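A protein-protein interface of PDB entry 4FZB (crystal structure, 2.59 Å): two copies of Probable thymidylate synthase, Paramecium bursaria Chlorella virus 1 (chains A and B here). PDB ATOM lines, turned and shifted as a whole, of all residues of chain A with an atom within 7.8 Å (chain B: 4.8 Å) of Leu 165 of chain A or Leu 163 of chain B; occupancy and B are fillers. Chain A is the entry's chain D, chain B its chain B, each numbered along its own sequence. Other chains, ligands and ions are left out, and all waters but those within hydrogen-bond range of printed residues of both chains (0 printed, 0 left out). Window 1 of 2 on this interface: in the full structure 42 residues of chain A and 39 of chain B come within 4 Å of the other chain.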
ATOM      1  N   THR A  73      22.319 -11.815 -16.151  1.00  0.00           N
ATOM      2  CA  THR A  73      22.827 -11.331 -17.429  1.00  0.00           C
ATOM      3  C   THR A  73      23.537 -12.443 -18.186  1.00  0.00           C
ATOM      4  O   THR A  73      23.446 -13.594 -17.767  1.00  0.00           O
ATOM      5  CB  THR A  73      23.625 -10.000 -17.224  1.00  0.00           C
ATOM      6  OG1 THR A  73      23.831  -9.382 -18.487  1.00  0.00           O
ATOM      7  CG2 THR A  73      24.951 -10.183 -16.498  1.00  0.00           C
ATOM      8  N   SER A  74      24.200 -12.106 -19.312  1.00  0.00           N
ATOM      9  CA  SER A  74      25.004 -12.998 -20.138  1.00  0.00           C
ATOM     10  C   SER A  74      26.478 -12.845 -19.758  1.00  0.00           C
ATOM     11  O   SER A  74      26.871 -11.812 -19.182  1.00  0.00           O
ATOM     12  CB  SER A  74      24.829 -12.665 -21.615  1.00  0.00           C
ATOM     13  OG  SER A  74      25.212 -11.332 -21.909  1.00  0.00           O
ATOM     14  N   ARG A  75      27.293 -13.888 -20.074  1.00  0.00           N
ATOM     15  CA  ARG A  75      28.727 -13.892 -19.782  1.00  0.00           C
ATOM     16  C   ARG A  75      29.458 -12.770 -20.483  1.00  0.00           C
ATOM     17  O   ARG A  75      30.457 -12.289 -19.955  1.00  0.00           O
ATOM     18  CB  ARG A  75      29.386 -15.247 -20.120  1.00  0.00           C
ATOM     19  CG  ARG A  75      29.252 -16.329 -19.042  1.00  0.00           C
ATOM     20  CD  ARG A  75      29.706 -15.909 -17.639  1.00  0.00           C
ATOM     21  NE  ARG A  75      31.067 -15.362 -17.602  1.00  0.00           N
ATOM     22  CZ  ARG A  75      31.600 -14.764 -16.542  1.00  0.00           C
ATOM     23  NH1 ARG A  75      32.842 -14.297 -16.591  1.00  0.00           N
ATOM     24  NH2 ARG A  75      30.897 -14.625 -15.428  1.00  0.00           N
ATOM     25  N   GLY A  76      28.951 -12.385 -21.659  1.00  0.00           N
ATOM     26  CA  GLY A  76      29.462 -11.318 -22.521  1.00  0.00           C
ATOM     27  C   GLY A  76      29.362  -9.953 -21.875  1.00  0.00           C
ATOM     28  O   GLY A  76      30.332  -9.192 -21.886  1.00  0.00           O
ATOM     29  N   ILE A  77      28.215  -9.663 -21.260  1.00  0.00           N
ATOM     30  CA  ILE A  77      27.974  -8.449 -20.494  1.00  0.00           C
ATOM     31  C   ILE A  77      28.753  -8.524 -19.169  1.00  0.00           C
ATOM     32  O   ILE A  77      29.418  -7.557 -18.838  1.00  0.00           O
ATOM     33  CB  ILE A  77      26.447  -8.201 -20.284  1.00  0.00           C
ATOM     34  CG1 ILE A  77      25.694  -7.989 -21.643  1.00  0.00           C
ATOM     35  CG2 ILE A  77      26.137  -7.089 -19.233  1.00  0.00           C
ATOM     36  CD1 ILE A  77      26.003  -6.623 -22.478  1.00  0.00           C
ATOM     37  N   ALA A  78      28.681  -9.659 -18.422  1.00  0.00           N
ATOM     38  CA  ALA A  78      29.371  -9.883 -17.124  1.00  0.00           C
ATOM     39  C   ALA A  78      30.818  -9.487 -17.179  1.00  0.00           C
ATOM     40  O   ALA A  78      31.362  -8.910 -16.241  1.00  0.00           O
ATOM     41  CB  ALA A  78      29.281 -11.342 -16.726  1.00  0.00           C
ATOM     42  N   ALA A  79      31.433  -9.820 -18.313  1.00  0.00           N
ATOM     43  CA  ALA A  79      32.802  -9.534 -18.692  1.00  0.00           C
ATOM     44  C   ALA A  79      33.031  -8.002 -18.676  1.00  0.00           C
ATOM     45  O   ALA A  79      34.077  -7.576 -18.197  1.00  0.00           O
ATOM     46  CB  ALA A  79      33.055 -10.102 -20.078  1.00  0.00           C
ATOM     47  N   PRO A 103      21.560 -21.222 -23.147  1.00  0.00           N
ATOM     48  CA  PRO A 103      21.739 -19.853 -23.643  1.00  0.00           C
ATOM     49  C   PRO A 103      20.701 -19.445 -24.684  1.00  0.00           C
ATOM     50  O   PRO A 103      20.393 -20.243 -25.577  1.00  0.00           O
ATOM     51  CB  PRO A 103      23.158 -19.875 -24.212  1.00  0.00           C
ATOM     52  CG  PRO A 103      23.852 -20.954 -23.475  1.00  0.00           C
ATOM     53  CD  PRO A 103      22.802 -22.006 -23.308  1.00  0.00           C
ATOM     54  N   HIS A 106      20.631 -13.839 -28.988  1.00  0.00           N
ATOM     55  CA  HIS A 106      20.850 -12.395 -28.845  1.00  0.00           C
ATOM     56  C   HIS A 106      20.422 -11.674 -30.105  1.00  0.00           C
ATOM     57  O   HIS A 106      20.486 -12.255 -31.183  1.00  0.00           O
ATOM     58  CB  HIS A 106      22.313 -12.077 -28.471  1.00  0.00           C
ATOM     59  CG  HIS A 106      22.533 -12.096 -26.993  1.00  0.00           C
ATOM     60  ND1 HIS A 106      22.598 -13.289 -26.285  1.00  0.00           N
ATOM     61  CD2 HIS A 106      22.608 -11.068 -26.120  1.00  0.00           C
ATOM     62  CE1 HIS A 106      22.738 -12.948 -25.018  1.00  0.00           C
ATOM     63  NE2 HIS A 106      22.761 -11.620 -24.868  1.00  0.00           N
ATOM     64  N   TRP A 131      19.987 -15.275 -37.855  1.00  0.00           N
ATOM     65  CA  TRP A 131      20.816 -15.111 -36.672  1.00  0.00           C
ATOM     66  C   TRP A 131      20.268 -15.817 -35.442  1.00  0.00           C
ATOM     67  O   TRP A 131      21.038 -16.472 -34.748  1.00  0.00           O
ATOM     68  CB  TRP A 131      21.040 -13.627 -36.405  1.00  0.00           C
ATOM     69  CG  TRP A 131      21.975 -13.326 -35.271  1.00  0.00           C
ATOM     70  CD1 TRP A 131      21.695 -12.579 -34.167  1.00  0.00           C
ATOM     71  CD2 TRP A 131      23.346 -13.726 -35.152  1.00  0.00           C
ATOM     72  NE1 TRP A 131      22.806 -12.477 -33.370  1.00  0.00           N
ATOM     73  CE2 TRP A 131      23.839 -13.173 -33.949  1.00  0.00           C
ATOM     74  CE3 TRP A 131      24.199 -14.548 -35.917  1.00  0.00           C
ATOM     75  CZ2 TRP A 131      25.152 -13.398 -33.503  1.00  0.00           C
ATOM     76  CZ3 TRP A 131      25.494 -14.772 -35.464  1.00  0.00           C
ATOM     77  CH2 TRP A 131      25.959 -14.191 -34.280  1.00  0.00           C
ATOM     78  N   LEU A 138      23.696 -23.648 -32.758  1.00  0.00           N
ATOM     79  CA  LEU A 138      25.026 -23.653 -32.187  1.00  0.00           C
ATOM     80  C   LEU A 138      24.969 -23.727 -30.680  1.00  0.00           C
ATOM     81  O   LEU A 138      25.752 -24.474 -30.088  1.00  0.00           O
ATOM     82  CB  LEU A 138      25.819 -22.427 -32.675  1.00  0.00           C
ATOM     83  CG  LEU A 138      27.288 -22.302 -32.207  1.00  0.00           C
ATOM     84  CD1 LEU A 138      28.154 -23.454 -32.724  1.00  0.00           C
ATOM     85  CD2 LEU A 138      27.886 -20.952 -32.601  1.00  0.00           C
ATOM     86  N   TYR A 139      24.010 -23.028 -30.054  1.00  0.00           N
ATOM     87  CA  TYR A 139      23.867 -23.070 -28.602  1.00  0.00           C
ATOM     88  C   TYR A 139      23.451 -24.420 -28.112  1.00  0.00           C
ATOM     89  O   TYR A 139      24.122 -24.926 -27.208  1.00  0.00           O
ATOM     90  CB  TYR A 139      22.992 -21.957 -28.028  1.00  0.00           C
ATOM     91  CG  TYR A 139      23.508 -20.557 -28.291  1.00  0.00           C
ATOM     92  CD1 TYR A 139      24.831 -20.334 -28.676  1.00  0.00           C
ATOM     93  CD2 TYR A 139      22.679 -19.450 -28.137  1.00  0.00           C
ATOM     94  CE1 TYR A 139      25.296 -19.051 -28.948  1.00  0.00           C
ATOM     95  CE2 TYR A 139      23.146 -18.160 -28.358  1.00  0.00           C
ATOM     96  CZ  TYR A 139      24.439 -17.969 -28.804  1.00  0.00           C
ATOM     97  OH  TYR A 139      24.866 -16.691 -29.034  1.00  0.00           O
ATOM     98  N   PHE A 161      34.595 -24.429 -21.043  1.00  0.00           N
ATOM     99  CA  PHE A 161      35.289 -23.805 -22.173  1.00  0.00           C
ATOM    100  C   PHE A 161      34.532 -23.819 -23.500  1.00  0.00           C
ATOM    101  O   PHE A 161      34.771 -22.937 -24.327  1.00  0.00           O
ATOM    102  CB  PHE A 161      36.719 -24.339 -22.331  1.00  0.00           C
ATOM    103  CG  PHE A 161      37.684 -23.764 -21.323  1.00  0.00           C
ATOM    104  CD1 PHE A 161      38.349 -22.568 -21.574  1.00  0.00           C
ATOM    105  CD2 PHE A 161      37.926 -24.415 -20.117  1.00  0.00           C
ATOM    106  CE1 PHE A 161      39.258 -22.047 -20.650  1.00  0.00           C
ATOM    107  CE2 PHE A 161      38.835 -23.888 -19.188  1.00  0.00           C
ATOM    108  CZ  PHE A 161      39.488 -22.702 -19.459  1.00  0.00           C
ATOM    109  N   ILE A 162      33.625 -24.797 -23.700  1.00  0.00           N
ATOM    110  CA  ILE A 162      32.790 -24.913 -24.913  1.00  0.00           C
ATOM    111  C   ILE A 162      31.515 -24.044 -24.831  1.00  0.00           C
ATOM    112  O   ILE A 162      30.809 -23.862 -25.838  1.00  0.00           O
ATOM    113  CB  ILE A 162      32.440 -26.383 -25.268  1.00  0.00           C
ATOM    114  CG1 ILE A 162      31.678 -27.086 -24.142  1.00  0.00           C
ATOM    115  CG2 ILE A 162      33.664 -27.154 -25.700  1.00  0.00           C
ATOM    116  CD1 ILE A 162      30.456 -27.594 -24.549  1.00  0.00           C
ATOM    117  N   LEU A 163      31.220 -23.544 -23.623  1.00  0.00           N
ATOM    118  CA  LEU A 163      30.065 -22.708 -23.352  1.00  0.00           C
ATOM    119  C   LEU A 163      30.252 -21.325 -23.995  1.00  0.00           C
ATOM    120  O   LEU A 163      31.371 -20.800 -23.970  1.00  0.00           O
ATOM    121  CB  LEU A 163      29.855 -22.593 -21.844  1.00  0.00           C
ATOM    122  CG  LEU A 163      28.757 -23.428 -21.183  1.00  0.00           C
ATOM    123  CD1 LEU A 163      28.498 -24.743 -21.903  1.00  0.00           C
ATOM    124  CD2 LEU A 163      29.080 -23.662 -19.753  1.00  0.00           C
ATOM    125  N   PRO A 164      29.198 -20.741 -24.625  1.00  0.00           N
ATOM    126  CA  PRO A 164      29.388 -19.450 -25.303  1.00  0.00           C
ATOM    127  C   PRO A 164      29.310 -18.197 -24.398  1.00  0.00           C
ATOM    128  O   PRO A 164      29.010 -18.282 -23.200  1.00  0.00           O
ATOM    129  CB  PRO A 164      28.287 -19.474 -26.356  1.00  0.00           C
ATOM    130  CG  PRO A 164      27.175 -20.227 -25.688  1.00  0.00           C
ATOM    131  CD  PRO A 164      27.818 -21.237 -24.790  1.00  0.00           C
ATOM    132  N   LEU A 165      29.552 -17.015 -24.994  1.00  0.00           N
ATOM    133  CA  LEU A 165      29.477 -15.738 -24.287  1.00  0.00           C
ATOM    134  C   LEU A 165      28.040 -15.324 -23.931  1.00  0.00           C
ATOM    135  O   LEU A 165      27.860 -14.499 -23.036  1.00  0.00           O
ATOM    136  CB  LEU A 165      30.228 -14.642 -25.069  1.00  0.00           C
ATOM    137  CG  LEU A 165      31.628 -14.275 -24.549  1.00  0.00           C
ATOM    138  CD1 LEU A 165      32.371 -15.476 -23.973  1.00  0.00           C
ATOM    139  CD2 LEU A 165      32.454 -13.647 -25.633  1.00  0.00           C
ATOM    140  N   SER A 166      27.027 -15.939 -24.591  1.00  0.00           N
ATOM    141  CA  SER A 166      25.583 -15.727 -24.372  1.00  0.00           C
ATOM    142  C   SER A 166      25.075 -16.444 -23.106  1.00  0.00           C
ATOM    143  O   SER A 166      23.945 -16.170 -22.683  1.00  0.00           O
ATOM    144  CB  SER A 166      24.788 -16.255 -25.566  1.00  0.00           C
ATOM    145  OG  SER A 166      25.019 -17.648 -25.737  1.00  0.00           O
ATOM    146  N   THR A 167      25.891 -17.398 -22.545  1.00  0.00           N
ATOM    147  CA  THR A 167      25.557 -18.197 -21.376  1.00  0.00           C
ATOM    148  C   THR A 167      25.058 -17.319 -20.246  1.00  0.00           C
ATOM    149  O   THR A 167      25.781 -16.399 -19.833  1.00  0.00           O
ATOM    150  CB  THR A 167      26.709 -19.098 -20.932  1.00  0.00           C
ATOM    151  OG1 THR A 167      27.090 -19.950 -21.999  1.00  0.00           O
ATOM    152  CG2 THR A 167      26.350 -19.956 -19.730  1.00  0.00           C
ATOM    153  N   PRO A 168      23.803 -17.582 -19.774  1.00  0.00           N
ATOM    154  CA  PRO A 168      23.240 -16.789 -18.681  1.00  0.00           C
ATOM    155  C   PRO A 168      24.073 -16.951 -17.422  1.00  0.00           C
ATOM    156  O   PRO A 168      24.666 -18.016 -17.186  1.00  0.00           O
ATOM    157  CB  PRO A 168      21.822 -17.358 -18.522  1.00  0.00           C
ATOM    158  CG  PRO A 168      21.523 -18.013 -19.833  1.00  0.00           C
ATOM    159  CD  PRO A 168      22.837 -18.618 -20.204  1.00  0.00           C
ATOM    160  N   THR A 169      24.180 -15.845 -16.667  1.00  0.00           N
ATOM    161  CA  THR A 169      24.966 -15.729 -15.447  1.00  0.00           C
ATOM    162  C   THR A 169      24.268 -14.895 -14.387  1.00  0.00           C
ATOM    163  O   THR A 169      23.638 -13.872 -14.684  1.00  0.00           O
ATOM    164  CB  THR A 169      26.412 -15.265 -15.760  1.00  0.00           C
ATOM    165  OG1 THR A 169      27.218 -15.372 -14.588  1.00  0.00           O
ATOM    166  CG2 THR A 169      26.494 -13.846 -16.327  1.00  0.00           C
ATOM    167  N   VAL B  99      38.274 -11.468 -33.691  1.00  0.00           N
ATOM    168  CA  VAL B  99      39.074 -12.651 -33.369  1.00  0.00           C
ATOM    169  C   VAL B  99      39.661 -13.303 -34.618  1.00  0.00           C
ATOM    170  O   VAL B  99      38.988 -14.097 -35.267  1.00  0.00           O
ATOM    171  CB  VAL B  99      38.285 -13.662 -32.495  1.00  0.00           C
ATOM    172  CG1 VAL B  99      39.222 -14.701 -31.881  1.00  0.00           C
ATOM    173  CG2 VAL B  99      37.491 -12.948 -31.407  1.00  0.00           C
ATOM    174  N   MET B 143      33.182 -20.413 -35.582  1.00  0.00           N
ATOM    175  CA  MET B 143      33.858 -19.471 -36.488  1.00  0.00           C
ATOM    176  C   MET B 143      33.113 -19.310 -37.804  1.00  0.00           C
ATOM    177  O   MET B 143      33.009 -18.182 -38.287  1.00  0.00           O
ATOM    178  CB  MET B 143      35.330 -19.840 -36.739  1.00  0.00           C
ATOM    179  CG  MET B 143      36.233 -19.607 -35.536  1.00  0.00           C
ATOM    180  SD  MET B 143      35.916 -18.058 -34.651  1.00  0.00           S
ATOM    181  CE  MET B 143      36.742 -16.850 -35.768  1.00  0.00           C
ATOM    182  N   TYR B 146      30.418 -17.061 -36.922  1.00  0.00           N
ATOM    183  CA  TYR B 146      31.023 -15.774 -36.562  1.00  0.00           C
ATOM    184  C   TYR B 146      31.370 -15.027 -37.818  1.00  0.00           C
ATOM    185  O   TYR B 146      30.809 -13.965 -38.045  1.00  0.00           O
ATOM    186  CB  TYR B 146      32.258 -15.952 -35.644  1.00  0.00           C
ATOM    187  CG  TYR B 146      32.924 -14.654 -35.234  1.00  0.00           C
ATOM    188  CD1 TYR B 146      33.995 -14.142 -35.952  1.00  0.00           C
ATOM    189  CD2 TYR B 146      32.472 -13.932 -34.134  1.00  0.00           C
ATOM    190  CE1 TYR B 146      34.594 -12.935 -35.596  1.00  0.00           C
ATOM    191  CE2 TYR B 146      33.062 -12.725 -33.764  1.00  0.00           C
ATOM    192  CZ  TYR B 146      34.121 -12.226 -34.503  1.00  0.00           C
ATOM    193  OH  TYR B 146      34.730 -11.044 -34.151  1.00  0.00           O
ATOM    194  N   ALA B 159      28.274 -10.376 -32.526  1.00  0.00           N
ATOM    195  CA  ALA B 159      28.930 -11.594 -33.013  1.00  0.00           C
ATOM    196  C   ALA B 159      29.804 -12.281 -31.943  1.00  0.00           C
ATOM    197  O   ALA B 159      30.170 -13.445 -32.104  1.00  0.00           O
ATOM    198  CB  ALA B 159      29.736 -11.304 -34.272  1.00  0.00           C
ATOM    199  N   ARG B 160      30.106 -11.569 -30.845  1.00  0.00           N
ATOM    200  CA  ARG B 160      30.872 -12.108 -29.731  1.00  0.00           C
ATOM    201  C   ARG B 160      30.025 -13.092 -28.941  1.00  0.00           C
ATOM    202  O   ARG B 160      30.573 -14.014 -28.350  1.00  0.00           O
ATOM    203  CB  ARG B 160      31.298 -10.994 -28.783  1.00  0.00           C
ATOM    204  CG  ARG B 160      32.602 -10.285 -29.113  1.00  0.00           C
ATOM    205  CD  ARG B 160      32.969  -9.282 -28.012  1.00  0.00           C
ATOM    206  NE  ARG B 160      31.797  -8.543 -27.507  1.00  0.00           N
ATOM    207  CZ  ARG B 160      31.198  -8.767 -26.336  1.00  0.00           C
ATOM    208  NH1 ARG B 160      30.124  -8.072 -25.991  1.00  0.00           N
ATOM    209  NH2 ARG B 160      31.666  -9.697 -25.509  1.00  0.00           N
ATOM    210  N   PHE B 161      28.708 -12.876 -28.884  1.00  0.00           N
ATOM    211  CA  PHE B 161      27.793 -13.714 -28.120  1.00  0.00           C
ATOM    212  C   PHE B 161      27.761 -15.206 -28.456  1.00  0.00           C
ATOM    213  O   PHE B 161      27.366 -16.007 -27.604  1.00  0.00           O
ATOM    214  CB  PHE B 161      26.397 -13.101 -28.060  1.00  0.00           C
ATOM    215  CG  PHE B 161      26.336 -11.926 -27.122  1.00  0.00           C
ATOM    216  CD1 PHE B 161      26.222 -12.117 -25.750  1.00  0.00           C
ATOM    217  CD2 PHE B 161      26.405 -10.629 -27.603  1.00  0.00           C
ATOM    218  CE1 PHE B 161      26.183 -11.027 -24.877  1.00  0.00           C
ATOM    219  CE2 PHE B 161      26.365  -9.541 -26.733  1.00  0.00           C
ATOM    220  CZ  PHE B 161      26.263  -9.745 -25.373  1.00  0.00           C
ATOM    221  N   ILE B 162      28.207 -15.583 -29.671  1.00  0.00           N
ATOM    222  CA  ILE B 162      28.295 -16.983 -30.110  1.00  0.00           C
ATOM    223  C   ILE B 162      29.663 -17.592 -29.745  1.00  0.00           C
ATOM    224  O   ILE B 162      29.830 -18.812 -29.801  1.00  0.00           O
ATOM    225  CB  ILE B 162      27.942 -17.181 -31.630  1.00  0.00           C
ATOM    226  CG1 ILE B 162      28.752 -16.291 -32.556  1.00  0.00           C
ATOM    227  CG2 ILE B 162      26.459 -17.054 -31.909  1.00  0.00           C
ATOM    228  CD1 ILE B 162      29.172 -16.993 -33.743  1.00  0.00           C
ATOM    229  N   LEU B 163      30.634 -16.738 -29.367  1.00  0.00           N
ATOM    230  CA  LEU B 163      32.006 -17.123 -29.062  1.00  0.00           C
ATOM    231  C   LEU B 163      32.171 -17.918 -27.750  1.00  0.00           C
ATOM    232  O   LEU B 163      31.605 -17.505 -26.739  1.00  0.00           O
ATOM    233  CB  LEU B 163      32.895 -15.871 -29.094  1.00  0.00           C
ATOM    234  CG  LEU B 163      33.849 -15.680 -30.292  1.00  0.00           C
ATOM    235  CD1 LEU B 163      33.316 -16.307 -31.587  1.00  0.00           C
ATOM    236  CD2 LEU B 163      34.150 -14.210 -30.505  1.00  0.00           C
ATOM    237  N   PRO B 164      32.941 -19.042 -27.735  1.00  0.00           N
ATOM    238  CA  PRO B 164      33.080 -19.821 -26.488  1.00  0.00           C
ATOM    239  C   PRO B 164      34.190 -19.350 -25.541  1.00  0.00           C
ATOM    240  O   PRO B 164      35.131 -18.680 -25.972  1.00  0.00           O
ATOM    241  CB  PRO B 164      33.370 -21.231 -27.002  1.00  0.00           C
ATOM    242  CG  PRO B 164      34.211 -20.986 -28.223  1.00  0.00           C
ATOM    243  CD  PRO B 164      33.671 -19.691 -28.846  1.00  0.00           C
ATOM    244  N   LEU B 165      34.117 -19.771 -24.249  1.00  0.00           N
ATOM    245  CA  LEU B 165      35.118 -19.426 -23.231  1.00  0.00           C
ATOM    246  C   LEU B 165      36.543 -19.784 -23.637  1.00  0.00           C
ATOM    247  O   LEU B 165      37.491 -19.133 -23.191  1.00  0.00           O
ATOM    248  CB  LEU B 165      34.783 -20.028 -21.853  1.00  0.00           C
ATOM    249  CG  LEU B 165      33.886 -19.218 -20.923  1.00  0.00           C
ATOM    250  CD1 LEU B 165      34.217 -17.718 -20.941  1.00  0.00           C
ATOM    251  CD2 LEU B 165      32.430 -19.450 -21.227  1.00  0.00           C
ATOM    252  N   THR B 167      37.824 -19.256 -26.535  1.00  0.00           N
ATOM    253  CA  THR B 167      38.314 -18.199 -27.435  1.00  0.00           C
ATOM    254  C   THR B 167      39.558 -17.499 -26.868  1.00  0.00           C
ATOM    255  O   THR B 167      39.572 -17.085 -25.698  1.00  0.00           O
ATOM    256  CB  THR B 167      37.191 -17.229 -27.856  1.00  0.00           C
ATOM    257  OG1 THR B 167      36.241 -17.963 -28.613  1.00  0.00           O
ATOM    258  CG2 THR B 167      37.695 -16.071 -28.715  1.00  0.00           C
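O of Phe 161 of chain B sits at hydrogen-bond distance from OH of Tyr 139 of chain A (3.0 Å). The backbone carbonyl oxygen (O) of Leu 163 of chain B lies within hydrogen-bond range of the backbone NH (N) of Leu 165 of chain A, at 2.7 Å. N of Leu 165 of chain B lies within hydrogen-bond range of O of Phe 161 of chain A. O of Leu 163 of chain A sits at hydrogen-bond distance from N of Leu 165 of chain B (2.9 Å). O of Phe 161 of chain B sits at hydrogen-bond distance from N of Ser 166 of chain A.
NE1 of Trp 131 of chain A is in hydrogen-bond range of O of His 106 of chain A (3.2 Å). The side-chain hydroxyl (OG1) of Thr 167 of chain B sits at hydrogen-bond distance from the backbone carbonyl oxygen (O) of Pro 164 of chain B, 3.0 Å away. The side-chain hydroxyl of Ser 166 of chain A sits close to the side-chain hydroxyl of Tyr 139 of chain A. O of Leu 165 of chain A is in hydrogen-bond range of N of Arg 75 of chain A (3.1 Å). N of Gly 76 of chain A sits at hydrogen-bond distance from O of Leu 165 of chain A, 2.7 Å away. The backbone NH of Ile 77 of chain A lies close to the side-chain hydroxyl of Ser 74 of chain A.
NH2 of Arg 160 of chain B touches O of Gly 76 of chain A, at 3.9 Å. Phe 161 of chain B touches His 106 of chain A. Phe 161 of chain A touches Pro 164 of chain B. Pro 164 of chain B touches Ile 162 of chain A. Leu 163 of chain A touches Pro 164 of chain B. Phe 161 of chain B touches Pro 164 of chain A. CB of Pro 164 of chain A touches O of Ile 162 of chain B, at 3.8 Å. CA of Pro 164 of chain A touches CA of Pro 164 of chain B, 3.9 Å away. Leu 165 of chain A touches Arg 160 of chain B. Phe 161 of chain B touches Leu 165 of chain A.
Leu 163 of chain B touches two residues of chain A. Of the printed residues of chain B, Tyr 139 of chain A touches Phe 161 and Ile 162. Of the printed residues of chain A, Phe 161 of chain B touches Ser 74, His 106, Tyr 139, Pro 164, Leu 165 and Ser 166. The nearest residue of chain B that does not touch Leu 165 of chain A is Leu 165 of chain B (4.2 Å). The nearest printed residue of chain B that does not touch Leu 163 of chain A is Leu 163 of chain B (4.3 Å).
Hydrophobic or aromatic side chains of chain B that line the printed part of chain A: Phe 161, Ile 162, Pro 164 and Leu 165. Among the printed residues, no Asp or Glu carboxylate lies within 4 Å of a Lys or Arg side-chain nitrogen of the other chain.
Phe 161 of chain A touches Leu 165 of chain B, and with the chains exchanged Leu 165 of chain A touches Phe 161 of chain B. Ile 162 of chain A touches Pro 164 of chain B, and with the chains exchanged Pro 164 of chain A touches Ile 162 of chain B. Leu 163 of chain A touches Leu 165 of chain B, and with the chains exchanged Leu 165 of chain A touches Leu 163 of chain B. Pro 164 of chain A touches its own counterpart, Pro 164 of chain B. Of the 20 pairs that touch across the chains among the printed residues, 11 have their exchanged pair printed and touching as well.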
